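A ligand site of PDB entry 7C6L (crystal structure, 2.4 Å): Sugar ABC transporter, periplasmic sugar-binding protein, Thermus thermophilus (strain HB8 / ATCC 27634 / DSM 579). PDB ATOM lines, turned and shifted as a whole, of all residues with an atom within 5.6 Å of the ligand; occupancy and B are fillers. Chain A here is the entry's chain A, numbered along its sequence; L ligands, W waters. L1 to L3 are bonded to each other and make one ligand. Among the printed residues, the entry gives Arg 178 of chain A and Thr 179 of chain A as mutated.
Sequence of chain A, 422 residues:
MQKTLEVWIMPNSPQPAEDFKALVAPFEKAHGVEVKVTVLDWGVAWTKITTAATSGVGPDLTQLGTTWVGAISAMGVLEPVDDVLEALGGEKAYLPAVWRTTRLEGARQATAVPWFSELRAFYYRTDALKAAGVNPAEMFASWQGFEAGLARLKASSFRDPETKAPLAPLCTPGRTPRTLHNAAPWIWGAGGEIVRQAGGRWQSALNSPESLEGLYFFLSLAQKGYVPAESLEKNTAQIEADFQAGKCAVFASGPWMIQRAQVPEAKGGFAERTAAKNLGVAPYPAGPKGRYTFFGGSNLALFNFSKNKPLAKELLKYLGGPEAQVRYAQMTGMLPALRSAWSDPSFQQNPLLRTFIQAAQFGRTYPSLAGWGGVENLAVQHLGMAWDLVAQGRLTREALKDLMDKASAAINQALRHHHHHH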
ATOM      1  N   PRO A  11      18.579  19.198 -11.627  1.00  0.00           N
ATOM      2  CA  PRO A  11      19.300  18.794 -12.835  1.00  0.00           C
ATOM      3  C   PRO A  11      19.921  17.386 -12.743  1.00  0.00           C
ATOM      4  O   PRO A  11      21.076  17.242 -12.434  1.00  0.00           O
ATOM      5  CB  PRO A  11      20.387  19.881 -12.971  1.00  0.00           C
ATOM      6  CG  PRO A  11      19.890  21.015 -12.090  1.00  0.00           C
ATOM      7  CD  PRO A  11      19.265  20.284 -10.914  1.00  0.00           C
ATOM      8  N   ASN A  12      19.107  16.379 -13.065  1.00  0.00           N
ATOM      9  CA  ASN A  12      19.392  14.953 -12.807  1.00  0.00           C
ATOM     10  C   ASN A  12      20.121  14.381 -14.014  1.00  0.00           C
ATOM     11  O   ASN A  12      20.787  13.345 -13.855  1.00  0.00           O
ATOM     12  CB  ASN A  12      18.094  14.173 -12.505  1.00  0.00           C
ATOM     13  CG  ASN A  12      17.391  14.673 -11.261  1.00  0.00           C
ATOM     14  OD1 ASN A  12      18.046  15.104 -10.303  1.00  0.00           O
ATOM     15  ND2 ASN A  12      16.080  14.603 -11.261  1.00  0.00           N
ATOM     16  N   SER A  13      19.948  15.002 -15.178  1.00  0.00           N
ATOM     17  CA  SER A  13      20.457  14.494 -16.490  1.00  0.00           C
ATOM     18  C   SER A  13      21.036  15.641 -17.286  1.00  0.00           C
ATOM     19  O   SER A  13      20.811  16.794 -16.938  1.00  0.00           O
ATOM     20  CB  SER A  13      19.365  13.820 -17.230  1.00  0.00           C
ATOM     21  OG  SER A  13      18.319  14.740 -17.574  1.00  0.00           O
ATOM     22  N   TRP A  42      20.092  22.689  -7.669  1.00  0.00           N
ATOM     23  CA  TRP A  42      20.250  22.176  -6.279  1.00  0.00           C
ATOM     24  C   TRP A  42      20.555  23.319  -5.319  1.00  0.00           C
ATOM     25  O   TRP A  42      20.022  23.305  -4.195  1.00  0.00           O
ATOM     26  CB  TRP A  42      21.332  21.098  -6.232  1.00  0.00           C
ATOM     27  CG  TRP A  42      20.866  19.738  -6.632  1.00  0.00           C
ATOM     28  CD1 TRP A  42      21.232  19.043  -7.753  1.00  0.00           C
ATOM     29  CD2 TRP A  42      19.967  18.888  -5.906  1.00  0.00           C
ATOM     30  NE1 TRP A  42      20.598  17.828  -7.782  1.00  0.00           N
ATOM     31  CE2 TRP A  42      19.846  17.681  -6.635  1.00  0.00           C
ATOM     32  CE3 TRP A  42      19.309  18.988  -4.680  1.00  0.00           C
ATOM     33  CZ2 TRP A  42      19.002  16.655  -6.245  1.00  0.00           C
ATOM     34  CZ3 TRP A  42      18.498  17.954  -4.254  1.00  0.00           C
ATOM     35  CH2 TRP A  42      18.324  16.806  -5.055  1.00  0.00           C
ATOM     36  N   GLN A  63      10.465  17.034  -6.801  1.00  0.00           N
ATOM     37  CA  GLN A  63      11.595  16.140  -6.416  1.00  0.00           C
ATOM     38  C   GLN A  63      12.060  16.632  -5.060  1.00  0.00           C
ATOM     39  O   GLN A  63      12.093  17.854  -4.893  1.00  0.00           O
ATOM     40  CB  GLN A  63      12.705  16.244  -7.451  1.00  0.00           C
ATOM     41  CG  GLN A  63      13.976  15.504  -7.074  1.00  0.00           C
ATOM     42  CD  GLN A  63      14.963  15.513  -8.215  1.00  0.00           C
ATOM     43  OE1 GLN A  63      14.681  15.983  -9.330  1.00  0.00           O
ATOM     44  NE2 GLN A  63      16.159  15.047  -7.939  1.00  0.00           N
ATOM     45  N   GLY A  65      15.332  15.646  -2.264  1.00  0.00           N
ATOM     46  CA  GLY A  65      16.477  14.837  -1.807  1.00  0.00           C
ATOM     47  C   GLY A  65      16.071  13.987  -0.622  1.00  0.00           C
ATOM     48  O   GLY A  65      15.408  14.497   0.258  1.00  0.00           O
ATOM     49  N   THR A  66      16.501  12.725  -0.585  1.00  0.00           N
ATOM     50  CA  THR A  66      16.206  11.783   0.524  1.00  0.00           C
ATOM     51  C   THR A  66      16.483  12.482   1.863  1.00  0.00           C
ATOM     52  O   THR A  66      15.691  12.314   2.792  1.00  0.00           O
ATOM     53  CB  THR A  66      16.980  10.487   0.365  1.00  0.00           C
ATOM     54  OG1 THR A  66      18.341  10.894   0.136  1.00  0.00           O
ATOM     55  CG2 THR A  66      16.437   9.658  -0.769  1.00  0.00           C
ATOM     56  N   THR A  67      17.504  13.301   1.935  1.00  0.00           N
ATOM     57  CA  THR A  67      17.895  13.885   3.238  1.00  0.00           C
ATOM     58  C   THR A  67      16.958  14.992   3.659  1.00  0.00           C
ATOM     59  O   THR A  67      17.094  15.427   4.754  1.00  0.00           O
ATOM     60  CB  THR A  67      19.359  14.361   3.263  1.00  0.00           C
ATOM     61  OG1 THR A  67      19.377  15.551   2.496  1.00  0.00           O
ATOM     62  CG2 THR A  67      20.299  13.265   2.808  1.00  0.00           C
ATOM     63  N   TRP A  68      16.090  15.439   2.784  1.00  0.00           N
ATOM     64  CA  TRP A  68      15.152  16.557   3.030  1.00  0.00           C
ATOM     65  C   TRP A  68      13.760  16.001   3.394  1.00  0.00           C
ATOM     66  O   TRP A  68      12.871  16.821   3.703  1.00  0.00           O
ATOM     67  CB  TRP A  68      15.078  17.471   1.798  1.00  0.00           C
ATOM     68  CG  TRP A  68      16.346  18.194   1.500  1.00  0.00           C
ATOM     69  CD1 TRP A  68      17.451  18.227   2.285  1.00  0.00           C
ATOM     70  CD2 TRP A  68      16.688  18.970   0.334  1.00  0.00           C
ATOM     71  NE1 TRP A  68      18.466  18.932   1.693  1.00  0.00           N
ATOM     72  CE2 TRP A  68      18.012  19.439   0.509  1.00  0.00           C
ATOM     73  CE3 TRP A  68      16.024  19.339  -0.809  1.00  0.00           C
ATOM     74  CZ2 TRP A  68      18.679  20.263  -0.408  1.00  0.00           C
ATOM     75  CZ3 TRP A  68      16.660  20.169  -1.718  1.00  0.00           C
ATOM     76  CH2 TRP A  68      17.964  20.620  -1.524  1.00  0.00           C
ATOM     77  N   PHE A 116      14.898   7.741  -7.527  1.00  0.00           N
ATOM     78  CA  PHE A 116      16.210   7.133  -7.851  1.00  0.00           C
ATOM     79  C   PHE A 116      17.149   7.212  -6.650  1.00  0.00           C
ATOM     80  O   PHE A 116      16.927   8.029  -5.748  1.00  0.00           O
ATOM     81  CB  PHE A 116      16.804   7.799  -9.097  1.00  0.00           C
ATOM     82  CG  PHE A 116      17.156   9.256  -8.914  1.00  0.00           C
ATOM     83  CD1 PHE A 116      18.339   9.622  -8.304  1.00  0.00           C
ATOM     84  CD2 PHE A 116      16.328  10.251  -9.402  1.00  0.00           C
ATOM     85  CE1 PHE A 116      18.672  10.953  -8.130  1.00  0.00           C
ATOM     86  CE2 PHE A 116      16.687  11.586  -9.266  1.00  0.00           C
ATOM     87  CZ  PHE A 116      17.860  11.929  -8.620  1.00  0.00           C
ATOM     88  N   GLU A 118      21.602   6.776  -5.470  1.00  0.00           N
ATOM     89  CA  GLU A 118      22.836   7.517  -5.802  1.00  0.00           C
ATOM     90  C   GLU A 118      23.782   7.210  -4.642  1.00  0.00           C
ATOM     91  O   GLU A 118      23.304   7.194  -3.527  1.00  0.00           O
ATOM     92  CB  GLU A 118      22.301   8.933  -5.859  1.00  0.00           C
ATOM     93  CG  GLU A 118      23.246  10.025  -6.089  1.00  0.00           C
ATOM     94  CD  GLU A 118      24.045  10.460  -4.895  1.00  0.00           C
ATOM     95  OE1 GLU A 118      23.561  11.360  -4.103  1.00  0.00           O
ATOM     96  OE2 GLU A 118      25.215   9.971  -4.858  1.00  0.00           O
ATOM     97  N   ARG A 120      28.361   7.277  -3.421  1.00  0.00           N
ATOM     98  CA  ARG A 120      29.609   7.960  -3.800  1.00  0.00           C
ATOM     99  C   ARG A 120      30.717   6.939  -3.896  1.00  0.00           C
ATOM    100  O   ARG A 120      30.689   5.971  -3.174  1.00  0.00           O
ATOM    101  CB  ARG A 120      29.921   9.114  -2.841  1.00  0.00           C
ATOM    102  CG  ARG A 120      28.780  10.111  -2.708  1.00  0.00           C
ATOM    103  CD  ARG A 120      28.343  10.637  -4.051  1.00  0.00           C
ATOM    104  NE  ARG A 120      27.098  11.403  -3.987  1.00  0.00           N
ATOM    105  CZ  ARG A 120      27.009  12.699  -3.753  1.00  0.00           C
ATOM    106  NH1 ARG A 120      28.065  13.433  -3.498  1.00  0.00           N
ATOM    107  NH2 ARG A 120      25.817  13.247  -3.715  1.00  0.00           N
ATOM    108  N   ARG A 178      28.029  22.841   0.544  1.00  0.00           N
ATOM    109  CA  ARG A 178      26.546  22.822   0.704  1.00  0.00           C
ATOM    110  C   ARG A 178      26.108  21.708   1.676  1.00  0.00           C
ATOM    111  O   ARG A 178      25.096  21.889   2.394  1.00  0.00           O
ATOM    112  CB  ARG A 178      25.863  22.537  -0.638  1.00  0.00           C
ATOM    113  CG  ARG A 178      25.727  23.739  -1.561  1.00  0.00           C
ATOM    114  CD  ARG A 178      24.491  23.598  -2.475  1.00  0.00           C
ATOM    115  NE  ARG A 178      24.583  22.528  -3.483  1.00  0.00           N
ATOM    116  CZ  ARG A 178      24.776  22.700  -4.783  1.00  0.00           C
ATOM    117  NH1 ARG A 178      24.919  23.916  -5.320  1.00  0.00           N
ATOM    118  NH2 ARG A 178      24.856  21.629  -5.548  1.00  0.00           N
ATOM    119  N   THR A 179      26.824  20.583   1.664  1.00  0.00           N
ATOM    120  CA  THR A 179      26.485  19.288   2.296  1.00  0.00           C
ATOM    121  C   THR A 179      27.735  18.635   2.896  1.00  0.00           C
ATOM    122  O   THR A 179      28.880  19.005   2.547  1.00  0.00           O
ATOM    123  CB  THR A 179      25.901  18.312   1.255  1.00  0.00           C
ATOM    124  OG1 THR A 179      26.930  17.994   0.304  1.00  0.00           O
ATOM    125  CG2 THR A 179      24.673  18.906   0.580  1.00  0.00           C
ATOM    126  N   HIS A 181      28.295  15.442   2.317  1.00  0.00           N
ATOM    127  CA  HIS A 181      28.400  14.204   1.520  1.00  0.00           C
ATOM    128  C   HIS A 181      29.892  13.789   1.411  1.00  0.00           C
ATOM    129  O   HIS A 181      30.191  12.546   1.518  1.00  0.00           O
ATOM    130  CB  HIS A 181      27.723  14.384   0.171  1.00  0.00           C
ATOM    131  CG  HIS A 181      26.284  14.760   0.251  1.00  0.00           C
ATOM    132  ND1 HIS A 181      25.542  14.609   1.415  1.00  0.00           N
ATOM    133  CD2 HIS A 181      25.445  15.277  -0.670  1.00  0.00           C
ATOM    134  CE1 HIS A 181      24.309  15.046   1.189  1.00  0.00           C
ATOM    135  NE2 HIS A 181      24.223  15.449  -0.093  1.00  0.00           N
ATOM    136  N   THR A 236      31.774  22.175  -5.771  1.00  0.00           N
ATOM    137  CA  THR A 236      31.568  20.852  -6.384  1.00  0.00           C
ATOM    138  C   THR A 236      31.510  20.965  -7.909  1.00  0.00           C
ATOM    139  O   THR A 236      32.136  20.128  -8.554  1.00  0.00           O
ATOM    140  CB  THR A 236      30.281  20.188  -5.872  1.00  0.00           C
ATOM    141  OG1 THR A 236      30.383  20.067  -4.445  1.00  0.00           O
ATOM    142  CG2 THR A 236      30.085  18.815  -6.491  1.00  0.00           C
ATOM    143  N   ALA A 237      30.745  21.898  -8.485  1.00  0.00           N
ATOM    144  CA  ALA A 237      30.554  21.951  -9.959  1.00  0.00           C
ATOM    145  C   ALA A 237      31.903  22.283 -10.602  1.00  0.00           C
ATOM    146  O   ALA A 237      32.211  21.766 -11.704  1.00  0.00           O
ATOM    147  CB  ALA A 237      29.462  22.922 -10.347  1.00  0.00           C
ATOM    148  N   GLU A 240      34.202  19.143 -10.477  1.00  0.00           N
ATOM    149  CA  GLU A 240      33.719  18.235 -11.536  1.00  0.00           C
ATOM    150  C   GLU A 240      34.345  18.655 -12.861  1.00  0.00           C
ATOM    151  O   GLU A 240      34.911  17.774 -13.553  1.00  0.00           O
ATOM    152  CB  GLU A 240      32.195  18.246 -11.663  1.00  0.00           C
ATOM    153  CG  GLU A 240      31.522  16.965 -11.177  1.00  0.00           C
ATOM    154  CD  GLU A 240      30.004  16.881 -11.296  1.00  0.00           C
ATOM    155  OE1 GLU A 240      29.407  17.707 -12.021  1.00  0.00           O
ATOM    156  OE2 GLU A 240      29.412  15.947 -10.687  1.00  0.00           O
ATOM    157  N   SER A 253      32.586  11.310  -6.580  1.00  0.00           N
ATOM    158  CA  SER A 253      31.251  11.759  -7.087  1.00  0.00           C
ATOM    159  C   SER A 253      30.292  10.574  -7.108  1.00  0.00           C
ATOM    160  O   SER A 253      30.642   9.510  -6.572  1.00  0.00           O
ATOM    161  CB  SER A 253      31.382  12.402  -8.435  1.00  0.00           C
ATOM    162  OG  SER A 253      30.191  13.084  -8.731  1.00  0.00           O
ATOM    163  N   TRP A 256      26.280   9.315 -11.859  1.00  0.00           N
ATOM    164  CA  TRP A 256      25.863  10.134 -13.021  1.00  0.00           C
ATOM    165  C   TRP A 256      27.081  10.452 -13.900  1.00  0.00           C
ATOM    166  O   TRP A 256      26.862  10.584 -15.124  1.00  0.00           O
ATOM    167  CB  TRP A 256      25.170  11.405 -12.584  1.00  0.00           C
ATOM    168  CG  TRP A 256      26.007  12.312 -11.755  1.00  0.00           C
ATOM    169  CD1 TRP A 256      26.866  13.271 -12.194  1.00  0.00           C
ATOM    170  CD2 TRP A 256      25.995  12.389 -10.320  1.00  0.00           C
ATOM    171  NE1 TRP A 256      27.417  13.913 -11.134  1.00  0.00           N
ATOM    172  CE2 TRP A 256      26.910  13.384  -9.965  1.00  0.00           C
ATOM    173  CE3 TRP A 256      25.317  11.695  -9.317  1.00  0.00           C
ATOM    174  CZ2 TRP A 256      27.099  13.755  -8.645  1.00  0.00           C
ATOM    175  CZ3 TRP A 256      25.541  12.023  -8.016  1.00  0.00           C
ATOM    176  CH2 TRP A 256      26.406  13.064  -7.691  1.00  0.00           C
ATOM    177  N   ARG A 260      27.588  10.866 -18.034  1.00  0.00           N
ATOM    178  CA  ARG A 260      28.126  12.121 -18.614  1.00  0.00           C
ATOM    179  C   ARG A 260      29.367  11.784 -19.434  1.00  0.00           C
ATOM    180  O   ARG A 260      29.620  12.451 -20.445  1.00  0.00           O
ATOM    181  CB  ARG A 260      28.425  13.164 -17.533  1.00  0.00           C
ATOM    182  CG  ARG A 260      27.239  13.593 -16.652  1.00  0.00           C
ATOM    183  CD  ARG A 260      26.017  14.218 -17.323  1.00  0.00           C
ATOM    184  NE  ARG A 260      25.014  14.561 -16.310  1.00  0.00           N
ATOM    185  CZ  ARG A 260      24.207  13.714 -15.673  1.00  0.00           C
ATOM    186  NH1 ARG A 260      24.105  12.428 -15.959  1.00  0.00           N
ATOM    187  NH2 ARG A 260      23.437  14.184 -14.728  1.00  0.00           N
ATOM    188  N   PHE A 294      28.461   7.541   1.500  1.00  0.00           N
ATOM    189  CA  PHE A 294      27.174   8.262   1.460  1.00  0.00           C
ATOM    190  C   PHE A 294      26.265   7.603   0.415  1.00  0.00           C
ATOM    191  O   PHE A 294      26.704   7.428  -0.737  1.00  0.00           O
ATOM    192  CB  PHE A 294      27.368   9.727   1.120  1.00  0.00           C
ATOM    193  CG  PHE A 294      26.036  10.409   0.954  1.00  0.00           C
ATOM    194  CD1 PHE A 294      25.303  10.733   2.078  1.00  0.00           C
ATOM    195  CD2 PHE A 294      25.537  10.713  -0.302  1.00  0.00           C
ATOM    196  CE1 PHE A 294      24.065  11.330   1.942  1.00  0.00           C
ATOM    197  CE2 PHE A 294      24.299  11.320  -0.435  1.00  0.00           C
ATOM    198  CZ  PHE A 294      23.573  11.620   0.667  1.00  0.00           C
ATOM    199  N   PHE A 295      25.083   7.174   0.843  1.00  0.00           N
ATOM    200  CA  PHE A 295      24.006   6.625  -0.029  1.00  0.00           C
ATOM    201  C   PHE A 295      22.824   7.589   0.096  1.00  0.00           C
ATOM    202  O   PHE A 295      22.359   7.839   1.234  1.00  0.00           O
ATOM    203  CB  PHE A 295      23.615   5.218   0.404  1.00  0.00           C
ATOM    204  CG  PHE A 295      22.631   4.503  -0.480  1.00  0.00           C
ATOM    205  CD1 PHE A 295      21.271   4.805  -0.441  1.00  0.00           C
ATOM    206  CD2 PHE A 295      23.039   3.435  -1.257  1.00  0.00           C
ATOM    207  CE1 PHE A 295      20.360   4.098  -1.224  1.00  0.00           C
ATOM    208  CE2 PHE A 295      22.132   2.732  -2.053  1.00  0.00           C
ATOM    209  CZ  PHE A 295      20.804   3.067  -2.048  1.00  0.00           C
ATOM    210  N   GLY A 296      22.358   8.138  -1.023  1.00  0.00           N
ATOM    211  CA  GLY A 296      21.196   9.043  -1.043  1.00  0.00           C
ATOM    212  C   GLY A 296      20.377   8.867  -2.304  1.00  0.00           C
ATOM    213  O   GLY A 296      20.047   7.733  -2.644  1.00  0.00           O
ATOM    214  N   GLY A 297      19.957   9.986  -2.904  1.00  0.00           N
ATOM    215  CA  GLY A 297      19.013   9.932  -4.013  1.00  0.00           C
ATOM    216  C   GLY A 297      17.867  10.878  -3.784  1.00  0.00           C
ATOM    217  O   GLY A 297      17.974  11.715  -2.950  1.00  0.00           O
ATOM    218  N   SER A 298      16.883  10.830  -4.655  1.00  0.00           N
ATOM    219  CA  SER A 298      15.725  11.749  -4.615  1.00  0.00           C
ATOM    220  C   SER A 298      14.456  10.914  -4.641  1.00  0.00           C
ATOM    221  O   SER A 298      14.474   9.763  -5.164  1.00  0.00           O
ATOM    222  CB  SER A 298      15.779  12.723  -5.729  1.00  0.00           C
ATOM    223  OG  SER A 298      16.877  13.593  -5.595  1.00  0.00           O
ATOM    224  N   MET A 334      21.803   7.619 -12.764  1.00  0.00           N
ATOM    225  CA  MET A 334      21.570   7.292 -11.348  1.00  0.00           C
ATOM    226  C   MET A 334      21.202   5.800 -11.247  1.00  0.00           C
ATOM    227  O   MET A 334      21.060   5.164 -12.270  1.00  0.00           O
ATOM    228  CB  MET A 334      20.440   8.152 -10.795  1.00  0.00           C
ATOM    229  CG  MET A 334      20.650   9.620 -11.036  1.00  0.00           C
ATOM    230  SD  MET A 334      21.954  10.243  -9.959  1.00  0.00           S
ATOM    231  CE  MET A 334      21.799  11.999 -10.294  1.00  0.00           C
ATOM    232  N   GLU A 376      22.578  20.010   8.861  1.00  0.00           N
ATOM    233  CA  GLU A 376      23.546  19.992   7.736  1.00  0.00           C
ATOM    234  C   GLU A 376      24.053  21.409   7.511  1.00  0.00           C
ATOM    235  O   GLU A 376      25.281  21.590   7.361  1.00  0.00           O
ATOM    236  CB  GLU A 376      22.918  19.358   6.487  1.00  0.00           C
ATOM    237  CG  GLU A 376      23.947  19.048   5.408  1.00  0.00           C
ATOM    238  CD  GLU A 376      23.701  17.743   4.656  1.00  0.00           C
ATOM    239  OE1 GLU A 376      22.516  17.472   4.356  1.00  0.00           O
ATOM    240  OE2 GLU A 376      24.697  17.054   4.330  1.00  0.00           O
HETATM  241  C1  LIG L   1      25.513  17.178 -12.549  1.00  0.00           C
HETATM  242  C2  LIG L   1      24.441  16.221 -12.009  1.00  0.00           C
HETATM  243  C3  LIG L   1      23.810  16.741 -10.706  1.00  0.00           C
HETATM  244  C4  LIG L   1      24.935  17.018  -9.718  1.00  0.00           C
HETATM  245  C5  LIG L   1      25.835  18.090 -10.377  1.00  0.00           C
HETATM  246  C6  LIG L   1      26.982  18.647  -9.544  1.00  0.00           C
HETATM  247  O1  LIG L   1      24.892  18.389 -12.891  1.00  0.00           O
HETATM  248  O2  LIG L   1      23.534  16.035 -13.090  1.00  0.00           O
HETATM  249  O3  LIG L   1      22.865  15.809 -10.176  1.00  0.00           O
HETATM  250  O4  LIG L   1      24.561  17.560  -8.441  1.00  0.00           O
HETATM  251  O5  LIG L   1      26.466  17.480 -11.525  1.00  0.00           O
HETATM  252  O6  LIG L   1      27.816  17.585  -9.076  1.00  0.00           O
HETATM  253  C1  LG2 L   2      23.848  16.896  -7.446  1.00  0.00           C
HETATM  254  C2  LG2 L   2      24.341  17.345  -6.081  1.00  0.00           C
HETATM  255  C3  LG2 L   2      23.162  17.092  -5.162  1.00  0.00           C
HETATM  256  C4  LG2 L   2      22.653  15.641  -5.310  1.00  0.00           C
HETATM  257  C5  LG2 L   2      23.397  14.785  -6.337  1.00  0.00           C
HETATM  258  C6  LG2 L   2      22.452  13.682  -6.867  1.00  0.00           C
HETATM  259  O1  LG2 L   2      24.716  18.715  -6.052  1.00  0.00           O
HETATM  260  O2  LG2 L   2      23.452  17.442  -3.811  1.00  0.00           O
HETATM  261  O3  LG2 L   2      22.786  14.892  -4.084  1.00  0.00           O
HETATM  262  O4  LG2 L   2      23.899  15.486  -7.520  1.00  0.00           O
HETATM  263  O5  LG2 L   2      21.086  14.060  -7.113  1.00  0.00           O
HETATM  264  C1  LG3 L   3      21.588  14.778  -3.355  1.00  0.00           C
HETATM  265  O1  LG3 L   3      21.602  15.915  -2.534  1.00  0.00           O
HETATM  266  C2  LG3 L   3      20.964  15.822  -1.251  1.00  0.00           C
HETATM  267  C3  LG3 L   3      20.533  17.208  -1.008  1.00  0.00           C
HETATM  268  O2  LG3 L   3      21.397  17.717  -0.034  1.00  0.00           O
HETATM  269  C4  LG3 L   3      19.814  14.834  -1.254  1.00  0.00           C
HETATM  270  O3  LG3 L   3      19.311  14.760   0.075  1.00  0.00           O
HETATM  271  C5  LG3 L   3      20.221  13.446  -1.743  1.00  0.00           C
HETATM  272  O4  LG3 L   3      20.405  12.512  -0.686  1.00  0.00           O
HETATM  273  C6  LG3 L   3      21.478  13.481  -2.573  1.00  0.00           C
HETATM  274  O5  LG3 L   3      21.356  12.383  -3.451  1.00  0.00           O
HETATM  275  O   HOH W   1      20.609  15.378  -9.348  1.00  0.00           O
HETATM  276  O   HOH W   2      26.755  19.742 -14.384  1.00  0.00           O
HETATM  277  O   HOH W   3      19.368  12.957  -5.465  1.00  0.00           O
HETATM  278  O   HOH W   4      22.285  20.180  -1.132  1.00  0.00           O
HETATM  279  O   HOH W   5      21.908  16.086   2.137  1.00  0.00           O
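OG1 of Thr 66 is in hydrogen-bond range of O4 of LG3 L3 (2.7 Å). The backbone NH (N) of Thr 67 lies within hydrogen-bond range of an oxygen (O3) of LG3 L3 (3.0 Å). The backbone carbonyl oxygen (O) of Gly 297 lies close to an oxygen (O4) of LG3 L3, 3.4 Å away. O6 of LIG L1 is in hydrogen-bond range of OE2 of Glu 240 (2.8 Å). The guanidinium group (NH2) of Arg 178 lies within hydrogen-bond range of an oxygen (O1) of LG2 L2 (3.0 Å). The guanidinium group (NH2) of Arg 260 lies within hydrogen-bond range of an oxygen (O2) of LIG L1, 2.5 Å away. The side-chain carboxylate (OE1) of Glu 118 is in hydrogen-bond range of an oxygen (O5) of LG3 L3, at 2.5 Å. O of Pro 11 is in hydrogen-bond range of O2 of LIG L1 (2.8 Å). O5 of LG3 L3 sits at hydrogen-bond distance from N of Gly 297, at 2.8 Å. NH2 of Arg 120 lies within hydrogen-bond range of O3 of LG2 L2, at 3.5 Å. The side-chain hydroxyl of Thr 67 is in hydrogen-bond range of an oxygen (O3) of LG3 L3 (2.5 Å).
The side-chain amide nitrogen (ND2) of Asn 12 sits at hydrogen-bond distance from the side-chain amide oxygen (OE1) of Gln 63. OE2 of Glu 240 is in hydrogen-bond range of NE1 of Trp 256 (2.9 Å). The side-chain carboxylate (OE2) of Glu 118 is in salt-bridge range of the guanidinium group (NE) of Arg 120, at 2.5 Å. N of Thr 66 lies within hydrogen-bond range of O of Gly 297. The guanidinium group (NH2) of Arg 260 lies within hydrogen-bond range of the backbone carbonyl oxygen (O) of Asn 12, 2.9 Å away. The backbone NH of Arg 120 lies within hydrogen-bond range of the backbone carbonyl oxygen of Phe 294, at 3.2 Å. NH1 of Arg 260 lies close to O of Trp 256, at 3.4 Å. The backbone carbonyl oxygen (O) of Glu 118 lies within hydrogen-bond range of the backbone NH (N) of Gly 296, 2.8 Å away.
C of Asn 12 touches O2 of LIG L1 (3.9 Å). Trp 42 touches the ligand. CA of Gly 65 touches C4 of LG3 L3, at 3.4 Å. NE1 of Trp 68 touches O2 of LG3 L3 (3.6 Å). Thr 179 touches the ligand. NE2 of His 181 touches C2 of LG3 L3 (3.5 Å). Thr 236 touches the ligand. CH2 of Trp 256 touches O4 of LG2 L2, 3.5 Å away. Phe 294 touches the ligand. CA of Gly 296 touches O4 of LG3 L3, at 3.6 Å. Met 334 touches the ligand. Hydrophobic or aromatic side chains within 4 Å of the ligand: Trp 42, Trp 68, Trp 256, Phe 294 and Met 334.
Water W1 lies within hydrogen-bond range of O3 of LIG L1 (2.4 Å), OD1 of Asn 12 (2.7 Å) and NE1 of Trp 42 (2.9 Å). Water W3 lies within hydrogen-bond range of OG of Ser 298 (2.6 Å), O5 of LG2 L2 (2.6 Å) and O of Gly 297 (3.1 Å). Water W5 lies within hydrogen-bond range of the side-chain hydroxyl (OG1) of Thr 67, the side-chain carboxylate (OE1) of Glu 376, an oxygen (O2) of LG3 L3 and a ring nitrogen (NE2) of His 181.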
